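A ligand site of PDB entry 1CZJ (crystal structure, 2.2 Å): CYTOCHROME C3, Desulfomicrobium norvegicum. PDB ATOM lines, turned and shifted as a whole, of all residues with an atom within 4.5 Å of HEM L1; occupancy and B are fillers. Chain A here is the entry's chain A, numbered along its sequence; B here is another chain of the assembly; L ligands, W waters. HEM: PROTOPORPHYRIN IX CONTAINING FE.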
ATOM      1  N   PHE A   3      19.693 -13.821 -26.785  1.00  0.00           N
ATOM      2  CA  PHE A   3      18.669 -12.916 -26.265  1.00  0.00           C
ATOM      3  C   PHE A   3      19.115 -11.466 -26.088  1.00  0.00           C
ATOM      4  O   PHE A   3      20.000 -11.198 -25.277  1.00  0.00           O
ATOM      5  CB  PHE A   3      18.170 -13.467 -24.917  1.00  0.00           C
ATOM      6  CG  PHE A   3      17.389 -12.471 -24.112  1.00  0.00           C
ATOM      7  CD1 PHE A   3      16.360 -11.718 -24.677  1.00  0.00           C
ATOM      8  CD2 PHE A   3      17.667 -12.287 -22.763  1.00  0.00           C
ATOM      9  CE1 PHE A   3      15.632 -10.819 -23.920  1.00  0.00           C
ATOM     10  CE2 PHE A   3      16.948 -11.397 -22.000  1.00  0.00           C
ATOM     11  CZ  PHE A   3      15.926 -10.659 -22.581  1.00  0.00           C
ATOM     12  N   ILE A   5      18.140  -7.489 -25.035  1.00  0.00           N
ATOM     13  CA  ILE A   5      17.231  -6.681 -24.240  1.00  0.00           C
ATOM     14  C   ILE A   5      17.073  -5.297 -24.856  1.00  0.00           C
ATOM     15  O   ILE A   5      18.046  -4.684 -25.286  1.00  0.00           O
ATOM     16  CB  ILE A   5      17.745  -6.495 -22.769  1.00  0.00           C
ATOM     17  CG1 ILE A   5      17.772  -7.827 -22.010  1.00  0.00           C
ATOM     18  CG2 ILE A   5      16.856  -5.517 -22.006  1.00  0.00           C
ATOM     19  CD1 ILE A   5      19.020  -8.640 -22.230  1.00  0.00           C
ATOM     20  N   PRO A   6      15.820  -4.814 -24.966  1.00  0.00           N
ATOM     21  CA  PRO A   6      15.549  -3.489 -25.519  1.00  0.00           C
ATOM     22  C   PRO A   6      15.775  -2.452 -24.415  1.00  0.00           C
ATOM     23  O   PRO A   6      15.151  -2.517 -23.354  1.00  0.00           O
ATOM     24  CB  PRO A   6      14.070  -3.571 -25.908  1.00  0.00           C
ATOM     25  CG  PRO A   6      13.512  -4.489 -24.860  1.00  0.00           C
ATOM     26  CD  PRO A   6      14.572  -5.574 -24.764  1.00  0.00           C
ATOM     27  N   VAL A   9      11.753   1.350 -24.126  1.00  0.00           N
ATOM     28  CA  VAL A   9      10.497   0.712 -24.484  1.00  0.00           C
ATOM     29  C   VAL A   9       9.363   1.725 -24.301  1.00  0.00           C
ATOM     30  O   VAL A   9       9.155   2.244 -23.205  1.00  0.00           O
ATOM     31  CB  VAL A   9      10.208  -0.514 -23.575  1.00  0.00           C
ATOM     32  CG1 VAL A   9       8.868  -1.113 -23.909  1.00  0.00           C
ATOM     33  CG2 VAL A   9      11.321  -1.556 -23.715  1.00  0.00           C
ATOM     34  N   MET A  11       5.787   2.282 -23.804  1.00  0.00           N
ATOM     35  CA  MET A  11       4.532   1.648 -23.429  1.00  0.00           C
ATOM     36  C   MET A  11       3.400   2.577 -23.844  1.00  0.00           C
ATOM     37  O   MET A  11       3.492   3.797 -23.646  1.00  0.00           O
ATOM     38  CB  MET A  11       4.514   1.399 -21.923  1.00  0.00           C
ATOM     39  CG  MET A  11       5.657   0.522 -21.462  1.00  0.00           C
ATOM     40  SD  MET A  11       5.705   0.277 -19.705  1.00  0.00           S
ATOM     41  CE  MET A  11       4.522  -1.035 -19.522  1.00  0.00           C
ATOM     42  N   PHE A  28       9.856   3.493 -20.966  1.00  0.00           N
ATOM     43  CA  PHE A  28      10.561   2.770 -19.915  1.00  0.00           C
ATOM     44  C   PHE A  28      12.002   2.502 -20.353  1.00  0.00           C
ATOM     45  O   PHE A  28      12.245   2.125 -21.499  1.00  0.00           O
ATOM     46  CB  PHE A  28       9.857   1.446 -19.582  1.00  0.00           C
ATOM     47  CG  PHE A  28      10.579   0.636 -18.553  1.00  0.00           C
ATOM     48  CD1 PHE A  28      10.592   1.044 -17.221  1.00  0.00           C
ATOM     49  CD2 PHE A  28      11.295  -0.487 -18.914  1.00  0.00           C
ATOM     50  CE1 PHE A  28      11.321   0.345 -16.263  1.00  0.00           C
ATOM     51  CE2 PHE A  28      12.031  -1.200 -17.971  1.00  0.00           C
ATOM     52  CZ  PHE A  28      12.046  -0.778 -16.638  1.00  0.00           C
ATOM     53  N   HIS A  30      15.489   0.443 -19.289  1.00  0.00           N
ATOM     54  CA  HIS A  30      16.081  -0.587 -18.458  1.00  0.00           C
ATOM     55  C   HIS A  30      17.375  -0.148 -17.748  1.00  0.00           C
ATOM     56  O   HIS A  30      17.625  -0.540 -16.618  1.00  0.00           O
ATOM     57  CB  HIS A  30      16.367  -1.848 -19.289  1.00  0.00           C
ATOM     58  CG  HIS A  30      15.175  -2.734 -19.486  1.00  0.00           C
ATOM     59  ND1 HIS A  30      14.418  -2.777 -20.640  1.00  0.00           N
ATOM     60  CD2 HIS A  30      14.632  -3.668 -18.669  1.00  0.00           C
ATOM     61  CE1 HIS A  30      13.476  -3.714 -20.486  1.00  0.00           C
ATOM     62  NE2 HIS A  30      13.564  -4.286 -19.312  1.00  0.00           N
ATOM     63  N   HIS A  33      17.120   1.006 -14.365  1.00  0.00           N
ATOM     64  CA  HIS A  33      16.548  -0.026 -13.509  1.00  0.00           C
ATOM     65  C   HIS A  33      17.404  -1.292 -13.480  1.00  0.00           C
ATOM     66  O   HIS A  33      17.025  -2.294 -12.867  1.00  0.00           O
ATOM     67  CB  HIS A  33      15.137  -0.362 -14.002  1.00  0.00           C
ATOM     68  CG  HIS A  33      14.199   0.799 -13.989  1.00  0.00           C
ATOM     69  ND1 HIS A  33      14.056   1.693 -15.027  1.00  0.00           N
ATOM     70  CD2 HIS A  33      13.374   1.254 -13.000  1.00  0.00           C
ATOM     71  CE1 HIS A  33      13.175   2.637 -14.651  1.00  0.00           C
ATOM     72  NE2 HIS A  33      12.738   2.415 -13.427  1.00  0.00           N
ATOM     73  N   MET A  34      18.592  -1.222 -14.077  1.00  0.00           N
ATOM     74  CA  MET A  34      19.460  -2.389 -14.177  1.00  0.00           C
ATOM     75  C   MET A  34      19.887  -3.088 -12.886  1.00  0.00           C
ATOM     76  O   MET A  34      20.284  -4.257 -12.923  1.00  0.00           O
ATOM     77  CB  MET A  34      20.690  -2.043 -15.034  1.00  0.00           C
ATOM     78  CG  MET A  34      21.482  -3.253 -15.536  1.00  0.00           C
ATOM     79  SD  MET A  34      20.517  -4.437 -16.515  1.00  0.00           S
ATOM     80  CE  MET A  34      20.269  -3.520 -18.034  1.00  0.00           C
ATOM     81  N   ILE A  36      17.879  -3.874 -10.463  1.00  0.00           N
ATOM     82  CA  ILE A  36      16.771  -4.652  -9.940  1.00  0.00           C
ATOM     83  C   ILE A  36      16.704  -5.969 -10.688  1.00  0.00           C
ATOM     84  O   ILE A  36      16.904  -6.007 -11.904  1.00  0.00           O
ATOM     85  CB  ILE A  36      15.435  -3.870 -10.063  1.00  0.00           C
ATOM     86  CG1 ILE A  36      15.555  -2.539  -9.312  1.00  0.00           C
ATOM     87  CG2 ILE A  36      14.277  -4.681  -9.489  1.00  0.00           C
ATOM     88  CD1 ILE A  36      14.705  -1.432  -9.888  1.00  0.00           C
ATOM     89  N   ALA A  37      16.477  -7.057  -9.952  1.00  0.00           N
ATOM     90  CA  ALA A  37      16.383  -8.396 -10.529  1.00  0.00           C
ATOM     91  C   ALA A  37      15.336  -8.428 -11.656  1.00  0.00           C
ATOM     92  O   ALA A  37      14.224  -7.924 -11.493  1.00  0.00           O
ATOM     93  CB  ALA A  37      16.018  -9.406  -9.455  1.00  0.00           C
ATOM     94  N   CYS A  38      15.706  -9.002 -12.792  1.00  0.00           N
ATOM     95  CA  CYS A  38      14.794  -9.083 -13.922  1.00  0.00           C
ATOM     96  C   CYS A  38      13.437  -9.669 -13.512  1.00  0.00           C
ATOM     97  O   CYS A  38      12.406  -9.038 -13.731  1.00  0.00           O
ATOM     98  CB  CYS A  38      15.371  -9.922 -15.060  1.00  0.00           C
ATOM     99  SG  CYS A  38      17.106  -9.587 -15.507  1.00  0.00           S
ATOM    100  N   CYS A  41      10.363  -7.565 -11.662  1.00  0.00           N
ATOM    101  CA  CYS A  41       9.347  -6.858 -12.445  1.00  0.00           C
ATOM    102  C   CYS A  41       8.640  -7.869 -13.320  1.00  0.00           C
ATOM    103  O   CYS A  41       7.414  -7.917 -13.352  1.00  0.00           O
ATOM    104  CB  CYS A  41       9.978  -5.761 -13.315  1.00  0.00           C
ATOM    105  SG  CYS A  41      10.652  -4.362 -12.379  1.00  0.00           S
ATOM    106  N   HIS A  42       9.425  -8.664 -14.047  1.00  0.00           N
ATOM    107  CA  HIS A  42       8.914  -9.702 -14.941  1.00  0.00           C
ATOM    108  C   HIS A  42       8.637 -10.899 -14.060  1.00  0.00           C
ATOM    109  O   HIS A  42       9.227 -11.973 -14.221  1.00  0.00           O
ATOM    110  CB  HIS A  42       9.942 -10.014 -16.030  1.00  0.00           C
ATOM    111  CG  HIS A  42      10.212  -8.858 -16.927  1.00  0.00           C
ATOM    112  ND1 HIS A  42       9.300  -8.352 -17.827  1.00  0.00           N
ATOM    113  CD2 HIS A  42      11.296  -8.046 -17.018  1.00  0.00           C
ATOM    114  CE1 HIS A  42       9.847  -7.262 -18.406  1.00  0.00           C
ATOM    115  NE2 HIS A  42      11.057  -7.039 -17.947  1.00  0.00           N
ATOM    116  N   ILE A  51       9.809 -13.729 -21.414  1.00  0.00           N
ATOM    117  CA  ILE A  51       9.656 -12.396 -20.874  1.00  0.00           C
ATOM    118  C   ILE A  51       8.732 -11.745 -21.883  1.00  0.00           C
ATOM    119  O   ILE A  51       9.015 -11.709 -23.087  1.00  0.00           O
ATOM    120  CB  ILE A  51      10.997 -11.626 -20.756  1.00  0.00           C
ATOM    121  CG1 ILE A  51      11.833 -12.202 -19.605  1.00  0.00           C
ATOM    122  CG2 ILE A  51      10.724 -10.136 -20.513  1.00  0.00           C
ATOM    123  CD1 ILE A  51      13.161 -11.529 -19.386  1.00  0.00           C
ATOM    124  N   GLU A  52       7.574 -11.291 -21.399  1.00  0.00           N
ATOM    125  CA  GLU A  52       6.588 -10.683 -22.263  1.00  0.00           C
ATOM    126  C   GLU A  52       6.004  -9.375 -21.730  1.00  0.00           C
ATOM    127  O   GLU A  52       6.198  -9.019 -20.553  1.00  0.00           O
ATOM    128  CB  GLU A  52       5.462 -11.688 -22.546  1.00  0.00           C
ATOM    129  CG  GLU A  52       4.790 -12.252 -21.284  1.00  0.00           C
ATOM    130  CD  GLU A  52       3.772 -13.350 -21.576  1.00  0.00           C
ATOM    131  OE1 GLU A  52       3.514 -13.662 -22.752  1.00  0.00           O
ATOM    132  OE2 GLU A  52       3.223 -13.913 -20.610  1.00  0.00           O
ATOM    133  N   SER A  53       5.284  -8.676 -22.597  1.00  0.00           N
ATOM    134  CA  SER A  53       4.636  -7.412 -22.253  1.00  0.00           C
ATOM    135  C   SER A  53       3.731  -7.562 -21.032  1.00  0.00           C
ATOM    136  O   SER A  53       3.070  -8.594 -20.881  1.00  0.00           O
ATOM    137  CB  SER A  53       3.809  -6.955 -23.463  1.00  0.00           C
ATOM    138  OG  SER A  53       3.071  -5.782 -23.182  1.00  0.00           O
ATOM    139  N   CYS A  54       3.698  -6.561 -20.149  1.00  0.00           N
ATOM    140  CA  CYS A  54       2.839  -6.650 -18.963  1.00  0.00           C
ATOM    141  C   CYS A  54       1.374  -6.619 -19.374  1.00  0.00           C
ATOM    142  O   CYS A  54       0.512  -7.232 -18.739  1.00  0.00           O
ATOM    143  CB  CYS A  54       3.051  -5.466 -18.010  1.00  0.00           C
ATOM    144  SG  CYS A  54       4.763  -4.963 -17.674  1.00  0.00           S
ATOM    145  N   MET A  55       1.107  -5.926 -20.466  1.00  0.00           N
ATOM    146  CA  MET A  55      -0.248  -5.761 -20.975  1.00  0.00           C
ATOM    147  C   MET A  55      -0.682  -6.810 -21.998  1.00  0.00           C
ATOM    148  O   MET A  55      -1.452  -6.515 -22.920  1.00  0.00           O
ATOM    149  CB  MET A  55      -0.379  -4.347 -21.555  1.00  0.00           C
ATOM    150  CG  MET A  55       0.114  -3.268 -20.585  1.00  0.00           C
ATOM    151  SD  MET A  55      -0.044  -1.591 -21.200  1.00  0.00           S
ATOM    152  CE  MET A  55       1.286  -1.531 -22.394  1.00  0.00           C
ATOM    153  N   THR B   2       8.857 -11.899 -26.212  1.00  0.00           N
ATOM    154  CA  THR B   2       9.150 -13.032 -27.155  1.00  0.00           C
ATOM    155  C   THR B   2      10.305 -13.927 -26.655  1.00  0.00           C
ATOM    156  O   THR B   2      10.376 -15.103 -27.005  1.00  0.00           O
ATOM    157  CB  THR B   2       9.490 -12.483 -28.575  1.00  0.00           C
ATOM    158  OG1 THR B   2       8.470 -11.556 -28.985  1.00  0.00           O
ATOM    159  CG2 THR B   2       9.583 -13.620 -29.593  1.00  0.00           C
ATOM    160  N   PHE B   3      11.173 -13.350 -25.826  1.00  0.00           N
ATOM    161  CA  PHE B   3      12.330 -14.041 -25.274  1.00  0.00           C
ATOM    162  C   PHE B   3      12.002 -15.318 -24.487  1.00  0.00           C
ATOM    163  O   PHE B   3      11.342 -15.247 -23.456  1.00  0.00           O
ATOM    164  CB  PHE B   3      13.105 -13.076 -24.373  1.00  0.00           C
ATOM    165  CG  PHE B   3      14.097 -13.752 -23.464  1.00  0.00           C
ATOM    166  CD1 PHE B   3      14.997 -14.691 -23.955  1.00  0.00           C
ATOM    167  CD2 PHE B   3      14.151 -13.422 -22.113  1.00  0.00           C
ATOM    168  CE1 PHE B   3      15.919 -15.303 -23.114  1.00  0.00           C
ATOM    169  CE2 PHE B   3      15.066 -14.018 -21.270  1.00  0.00           C
ATOM    170  CZ  PHE B   3      15.955 -14.956 -21.774  1.00  0.00           C
ATOM    171  N   GLN B  39      20.642 -11.418 -13.620  1.00  0.00           N
ATOM    172  CA  GLN B  39      21.914 -10.743 -13.780  1.00  0.00           C
ATOM    173  C   GLN B  39      22.991 -11.103 -12.734  1.00  0.00           C
ATOM    174  O   GLN B  39      24.148 -10.739 -12.907  1.00  0.00           O
ATOM    175  CB  GLN B  39      21.751  -9.224 -13.908  1.00  0.00           C
ATOM    176  CG  GLN B  39      21.132  -8.503 -12.725  1.00  0.00           C
ATOM    177  CD  GLN B  39      19.641  -8.327 -12.866  1.00  0.00           C
ATOM    178  OE1 GLN B  39      18.881  -9.283 -12.800  1.00  0.00           O
ATOM    179  NE2 GLN B  39      19.201  -7.088 -13.054  1.00  0.00           N
ATOM    180  N   VAL B  45      25.290  -8.620 -18.457  1.00  0.00           N
ATOM    181  CA  VAL B  45      24.142  -8.105 -19.194  1.00  0.00           C
ATOM    182  C   VAL B  45      24.223  -6.586 -19.414  1.00  0.00           C
ATOM    183  O   VAL B  45      23.918  -6.102 -20.504  1.00  0.00           O
ATOM    184  CB  VAL B  45      22.795  -8.453 -18.497  1.00  0.00           C
ATOM    185  CG1 VAL B  45      21.656  -7.693 -19.166  1.00  0.00           C
ATOM    186  CG2 VAL B  45      22.523  -9.946 -18.606  1.00  0.00           C
HETATM  187  CHA HEM L   1      10.366  -5.040 -21.338  1.00  0.00           C
HETATM  188  CHB HEM L   1      13.932  -8.178 -20.362  1.00  0.00           C
HETATM  189  CHC HEM L   1      14.604  -6.058 -16.084  1.00  0.00           C
HETATM  190  CHD HEM L   1      10.396  -3.781 -16.740  1.00  0.00           C
HETATM  191  C1A HEM L   1      11.304  -6.029 -21.473  1.00  0.00           C
HETATM  192  C2A HEM L   1      11.471  -6.866 -22.661  1.00  0.00           C
HETATM  193  C3A HEM L   1      12.460  -7.748 -22.322  1.00  0.00           C
HETATM  194  C4A HEM L   1      12.899  -7.478 -21.002  1.00  0.00           C
HETATM  195  CMA HEM L   1      13.018  -8.845 -23.194  1.00  0.00           C
HETATM  196  CAA HEM L   1      10.631  -6.910 -23.943  1.00  0.00           C
HETATM  197  CBA HEM L   1       9.562  -7.989 -23.745  1.00  0.00           C
HETATM  198  CGA HEM L   1       8.728  -8.245 -24.980  1.00  0.00           C
HETATM  199  O1A HEM L   1       7.709  -7.554 -25.159  1.00  0.00           O
HETATM  200  O2A HEM L   1       9.084  -9.176 -25.764  1.00  0.00           O
HETATM  201  C1B HEM L   1      14.449  -7.886 -19.104  1.00  0.00           C
HETATM  202  C2B HEM L   1      15.620  -8.503 -18.513  1.00  0.00           C
HETATM  203  C3B HEM L   1      15.873  -7.830 -17.367  1.00  0.00           C
HETATM  204  C4B HEM L   1      14.814  -6.839 -17.221  1.00  0.00           C
HETATM  205  CMB HEM L   1      16.413  -9.683 -19.041  1.00  0.00           C
HETATM  206  CAB HEM L   1      17.024  -7.983 -16.369  1.00  0.00           C
HETATM  207  CBB HEM L   1      18.414  -7.547 -16.857  1.00  0.00           C
HETATM  208  C1C HEM L   1      13.521  -5.203 -15.896  1.00  0.00           C
HETATM  209  C2C HEM L   1      13.197  -4.591 -14.655  1.00  0.00           C
HETATM  210  C3C HEM L   1      11.995  -3.998 -14.804  1.00  0.00           C
HETATM  211  C4C HEM L   1      11.586  -4.234 -16.174  1.00  0.00           C
HETATM  212  CMC HEM L   1      13.995  -4.649 -13.355  1.00  0.00           C
HETATM  213  CAC HEM L   1      11.186  -3.250 -13.738  1.00  0.00           C
HETATM  214  CBC HEM L   1      11.740  -1.923 -13.210  1.00  0.00           C
HETATM  215  C1D HEM L   1      10.036  -3.912 -18.064  1.00  0.00           C
HETATM  216  C2D HEM L   1       8.937  -3.204 -18.669  1.00  0.00           C
HETATM  217  C3D HEM L   1       8.979  -3.514 -19.992  1.00  0.00           C
HETATM  218  C4D HEM L   1      10.110  -4.382 -20.191  1.00  0.00           C
HETATM  219  CMD HEM L   1       7.906  -2.330 -17.972  1.00  0.00           C
HETATM  220  CAD HEM L   1       7.925  -3.088 -20.992  1.00  0.00           C
HETATM  221  CBD HEM L   1       6.804  -4.127 -20.965  1.00  0.00           C
HETATM  222  CGD HEM L   1       5.677  -3.815 -21.932  1.00  0.00           C
HETATM  223  O1D HEM L   1       4.515  -4.117 -21.582  1.00  0.00           O
HETATM  224  O2D HEM L   1       5.935  -3.281 -23.039  1.00  0.00           O
HETATM  225  NA  HEM L   1      12.171  -6.422 -20.461  1.00  0.00           N
HETATM  226  NB  HEM L   1      13.943  -6.871 -18.308  1.00  0.00           N
HETATM  227  NC  HEM L   1      12.524  -4.996 -16.840  1.00  0.00           N
HETATM  228  ND  HEM L   1      10.761  -4.619 -19.013  1.00  0.00           N
HETATM  229 FE   HEM L   1      12.373  -5.698 -18.666  1.00  0.00          FE
HETATM  230  CHA HEM L   2      13.844   5.869 -12.460  1.00  0.00           C
HETATM  231  CHB HEM L   2       9.881   4.774 -14.993  1.00  0.00           C
HETATM  232  CHC HEM L   2       9.277   0.820 -12.311  1.00  0.00           C
HETATM  233  CHD HEM L   2      12.940   2.189  -9.483  1.00  0.00           C
HETATM  234  C1A HEM L   2      12.756   5.947 -13.327  1.00  0.00           C
HETATM  235  C2A HEM L   2      12.537   6.991 -14.304  1.00  0.00           C
HETATM  236  C3A HEM L   2      11.398   6.692 -14.967  1.00  0.00           C
HETATM  237  C4A HEM L   2      10.930   5.465 -14.435  1.00  0.00           C
HETATM  238  CMA HEM L   2      10.677   7.532 -16.037  1.00  0.00           C
HETATM  239  CAA HEM L   2      13.423   8.200 -14.576  1.00  0.00           C
HETATM  240  CBA HEM L   2      14.656   7.887 -15.426  1.00  0.00           C
HETATM  241  CGA HEM L   2      14.295   7.188 -16.714  1.00  0.00           C
HETATM  242  O1A HEM L   2      14.853   6.104 -16.980  1.00  0.00           O
HETATM  243  O2A HEM L   2      13.428   7.701 -17.468  1.00  0.00           O
HETATM  244  C1B HEM L   2       9.403   3.588 -14.520  1.00  0.00           C
HETATM  245  C2B HEM L   2       8.243   2.915 -15.096  1.00  0.00           C
HETATM  246  C3B HEM L   2       8.031   1.853 -14.239  1.00  0.00           C
HETATM  247  C4B HEM L   2       9.099   1.827 -13.238  1.00  0.00           C
HETATM  248  CMB HEM L   2       7.430   3.342 -16.323  1.00  0.00           C
HETATM  249  CAB HEM L   2       6.906   0.811 -14.261  1.00  0.00           C
HETATM  250  CBB HEM L   2       6.887  -0.081 -15.508  1.00  0.00           C
HETATM  251  C1C HEM L   2      10.212   0.854 -11.294  1.00  0.00           C
HETATM  252  C2C HEM L   2      10.237  -0.071 -10.177  1.00  0.00           C
HETATM  253  C3C HEM L   2      11.223   0.333  -9.358  1.00  0.00           C
HETATM  254  C4C HEM L   2      11.835   1.503  -9.993  1.00  0.00           C
HETATM  255  CMC HEM L   2       9.214  -1.175  -9.900  1.00  0.00           C
HETATM  256  CAC HEM L   2      11.658  -0.199  -8.012  1.00  0.00           C
HETATM  257  CBC HEM L   2      11.733  -1.689  -7.689  1.00  0.00           C
HETATM  258  C1D HEM L   2      13.560   3.257 -10.112  1.00  0.00           C
HETATM  259  C2D HEM L   2      14.837   3.797  -9.713  1.00  0.00           C
HETATM  260  C3D HEM L   2      15.112   4.862 -10.547  1.00  0.00           C
HETATM  261  C4D HEM L   2      14.014   4.926 -11.492  1.00  0.00           C
HETATM  262  CMD HEM L   2      15.737   3.223  -8.632  1.00  0.00           C
HETATM  263  CAD HEM L   2      16.393   5.696 -10.404  1.00  0.00           C
HETATM  264  CBD HEM L   2      16.204   7.202 -10.154  1.00  0.00           C
HETATM  265  CGD HEM L   2      17.395   7.856  -9.447  1.00  0.00           C
HETATM  266  O1D HEM L   2      17.177   8.621  -8.481  1.00  0.00           O
HETATM  267  O2D HEM L   2      18.547   7.591  -9.853  1.00  0.00           O
HETATM  268  NA  HEM L   2      11.723   5.016 -13.385  1.00  0.00           N
HETATM  269  NB  HEM L   2       9.921   2.915 -13.378  1.00  0.00           N
HETATM  270  NC  HEM L   2      11.170   1.848 -11.154  1.00  0.00           N
HETATM  271  ND  HEM L   2      13.071   3.912 -11.244  1.00  0.00           N
HETATM  272 FE   HEM L   2      11.462   3.450 -12.241  1.00  0.00          FE
HETATM  273  CHA HEM L   3       0.201  -9.245 -10.122  1.00  0.00           C
HETATM  274  CHB HEM L   3       2.856  -5.766 -12.122  1.00  0.00           C
HETATM  275  CHC HEM L   3       3.519  -8.711 -15.918  1.00  0.00           C
HETATM  276  CHD HEM L   3       0.084 -11.615 -14.290  1.00  0.00           C
HETATM  277  C1A HEM L   3       0.844  -8.062 -10.360  1.00  0.00           C
HETATM  278  C2A HEM L   3       0.769  -6.903  -9.498  1.00  0.00           C
HETATM  279  C3A HEM L   3       1.498  -5.913 -10.043  1.00  0.00           C
HETATM  280  C4A HEM L   3       1.993  -6.455 -11.287  1.00  0.00           C
HETATM  281  CMA HEM L   3       1.663  -4.506  -9.460  1.00  0.00           C
HETATM  282  CAA HEM L   3      -0.066  -6.715  -8.236  1.00  0.00           C
HETATM  283  CBA HEM L   3       0.353  -7.509  -7.009  1.00  0.00           C
HETATM  284  CGA HEM L   3      -0.390  -7.090  -5.752  1.00  0.00           C
HETATM  285  O1A HEM L   3      -1.570  -6.660  -5.858  1.00  0.00           O
HETATM  286  O2A HEM L   3       0.200  -7.199  -4.644  1.00  0.00           O
HETATM  287  C1B HEM L   3       3.269  -6.263 -13.335  1.00  0.00           C
HETATM  288  C2B HEM L   3       4.148  -5.557 -14.227  1.00  0.00           C
HETATM  289  C3B HEM L   3       4.380  -6.390 -15.271  1.00  0.00           C
HETATM  290  C4B HEM L   3       3.591  -7.603 -15.043  1.00  0.00           C
HETATM  291  CMB HEM L   3       4.699  -4.151 -14.049  1.00  0.00           C
HETATM  292  CAB HEM L   3       5.312  -6.211 -16.456  1.00  0.00           C
HETATM  293  CBB HEM L   3       6.790  -6.056 -16.076  1.00  0.00           C
HETATM  294  C1C HEM L   3       2.672  -9.800 -15.825  1.00  0.00           C
HETATM  295  C2C HEM L   3       2.388 -10.736 -16.924  1.00  0.00           C
HETATM  296  C3C HEM L   3       1.294 -11.473 -16.521  1.00  0.00           C
HETATM  297  C4C HEM L   3       1.012 -11.041 -15.133  1.00  0.00           C
HETATM  298  CMC HEM L   3       3.110 -10.795 -18.273  1.00  0.00           C
HETATM  299  CAC HEM L   3       0.516 -12.513 -17.356  1.00  0.00           C
HETATM  300  CBC HEM L   3       1.257 -13.832 -17.606  1.00  0.00           C
HETATM  301  C1D HEM L   3      -0.204 -11.226 -12.997  1.00  0.00           C
HETATM  302  C2D HEM L   3      -1.088 -11.910 -12.081  1.00  0.00           C
HETATM  303  C3D HEM L   3      -1.011 -11.295 -10.889  1.00  0.00           C
HETATM  304  C4D HEM L   3      -0.081 -10.205 -11.067  1.00  0.00           C
HETATM  305  CMD HEM L   3      -1.905 -13.133 -12.429  1.00  0.00           C
HETATM  306  CAD HEM L   3      -1.659 -11.653  -9.557  1.00  0.00           C
HETATM  307  CBD HEM L   3      -1.317 -13.043  -9.029  1.00  0.00           C
HETATM  308  CGD HEM L   3       0.180 -13.320  -8.988  1.00  0.00           C
HETATM  309  O1D HEM L   3       0.916 -12.565  -8.299  1.00  0.00           O
HETATM  310  O2D HEM L   3       0.633 -14.301  -9.643  1.00  0.00           O
HETATM  311  NA  HEM L   3       1.533  -7.757 -11.508  1.00  0.00           N
HETATM  312  NB  HEM L   3       2.899  -7.509 -13.851  1.00  0.00           N
HETATM  313  NC  HEM L   3       1.821  -9.978 -14.739  1.00  0.00           N
HETATM  314  ND  HEM L   3       0.407 -10.164 -12.359  1.00  0.00           N
HETATM  315 FE   HEM L   3       1.714  -8.885 -13.089  1.00  0.00          FE
HETATM  316  O   HOH W   1      16.155  -2.941 -16.221  1.00  0.00           O
HETATM  317  O   HOH W   2      16.994  -4.770 -14.146  1.00  0.00           O
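Water W2 lies within hydrogen-bond range of the backbone carbonyl oxygen (O) of Ile 36 (2.6 Å), the backbone carbonyl oxygen (O) of His 33 (2.8 Å) and the side-chain amide nitrogen (NE2) of Gln 39 of chain B (3.4 Å).
The backbone NH (N) of Cys 38 lies within hydrogen-bond range of the side-chain amide oxygen (OE1) of Gln 39 of chain B. A ring nitrogen (ND1) of His 30 is in hydrogen-bond range of the backbone carbonyl oxygen (O) of Pro 6, 2.8 Å away. The backbone NH (N) of Met 55 lies close to the side-chain hydroxyl (OG) of Ser 53. The backbone NH of Thr 2 of chain B sits at hydrogen-bond distance from the backbone carbonyl oxygen of Ile 51 (3.1 Å). The backbone NH (N) of Phe 28 sits at hydrogen-bond distance from the backbone carbonyl oxygen (O) of Val 9 (2.7 Å). N of Ile 51 sits at hydrogen-bond distance from O of Phe 3 of chain B, at 3.0 Å. NE2 of Gln 39 of chain B sits at hydrogen-bond distance from O of Ile 36. The side-chain amide nitrogen (NE2) of Gln 39 of chain B lies within hydrogen-bond range of the backbone carbonyl oxygen (O) of Met 34, at 3.0 Å.
SG of Cys 38 is covalently linked to CAB of HEM L1 (1.8 Å). A carbon (CAC) of HEM L1 is covalently linked to the side-chain sulfur of Cys 41, 1.8 Å away. NE2 of His 30 is bound to FE of HEM L1, at 2.0 Å. A ring nitrogen (NE2) of His 42 binds an iron atom (FE) of HEM L1 (2.0 Å). OG of Ser 53 sits at hydrogen-bond distance from O1D of HEM L1 (2.7 Å). The backbone NH of Thr 2 of chain B sits at hydrogen-bond distance from an oxygen (O2A) of HEM L1 (2.8 Å). The backbone NH of Cys 54 lies within hydrogen-bond range of an oxygen (O1D) of HEM L1, at 2.9 Å. A ring nitrogen (NE2) of His 33 binds an iron atom (FE) of HEM L2 (2.0 Å). SG of Cys 54 is covalently linked to CAB of HEM L3.
Merely in contact with HEM L1: Phe 28, Phe 3 of chain A, Ile 51, Ile 36, His 33, Val 9, Met 11, Ile 5, Met 34, Ala 37, Pro 6, Gln 39 of chain B and Val 45 of chain B. Hydrophobic or aromatic side chains within 4 Å of HEM L1: Phe 3 of chain A, Ile 5, Pro 6, Val 9, Met 11, Phe 28, His 30, His 33, Met 34, Ile 36, His 42, Ile 51 and Val 45 of chain B. Within 4 Å of HEM L1: Phe 3 of chain A, Ile 5, Pro 6, Val 9, Met 11, Phe 28, His 30, His 33, Met 34, Ile 36, Ala 37, Cys 38, Cys 41, His 42, Ile 51, Ser 53, Cys 54, Thr 2 of chain B, Gln 39 of chain B and Val 45 of chain B.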
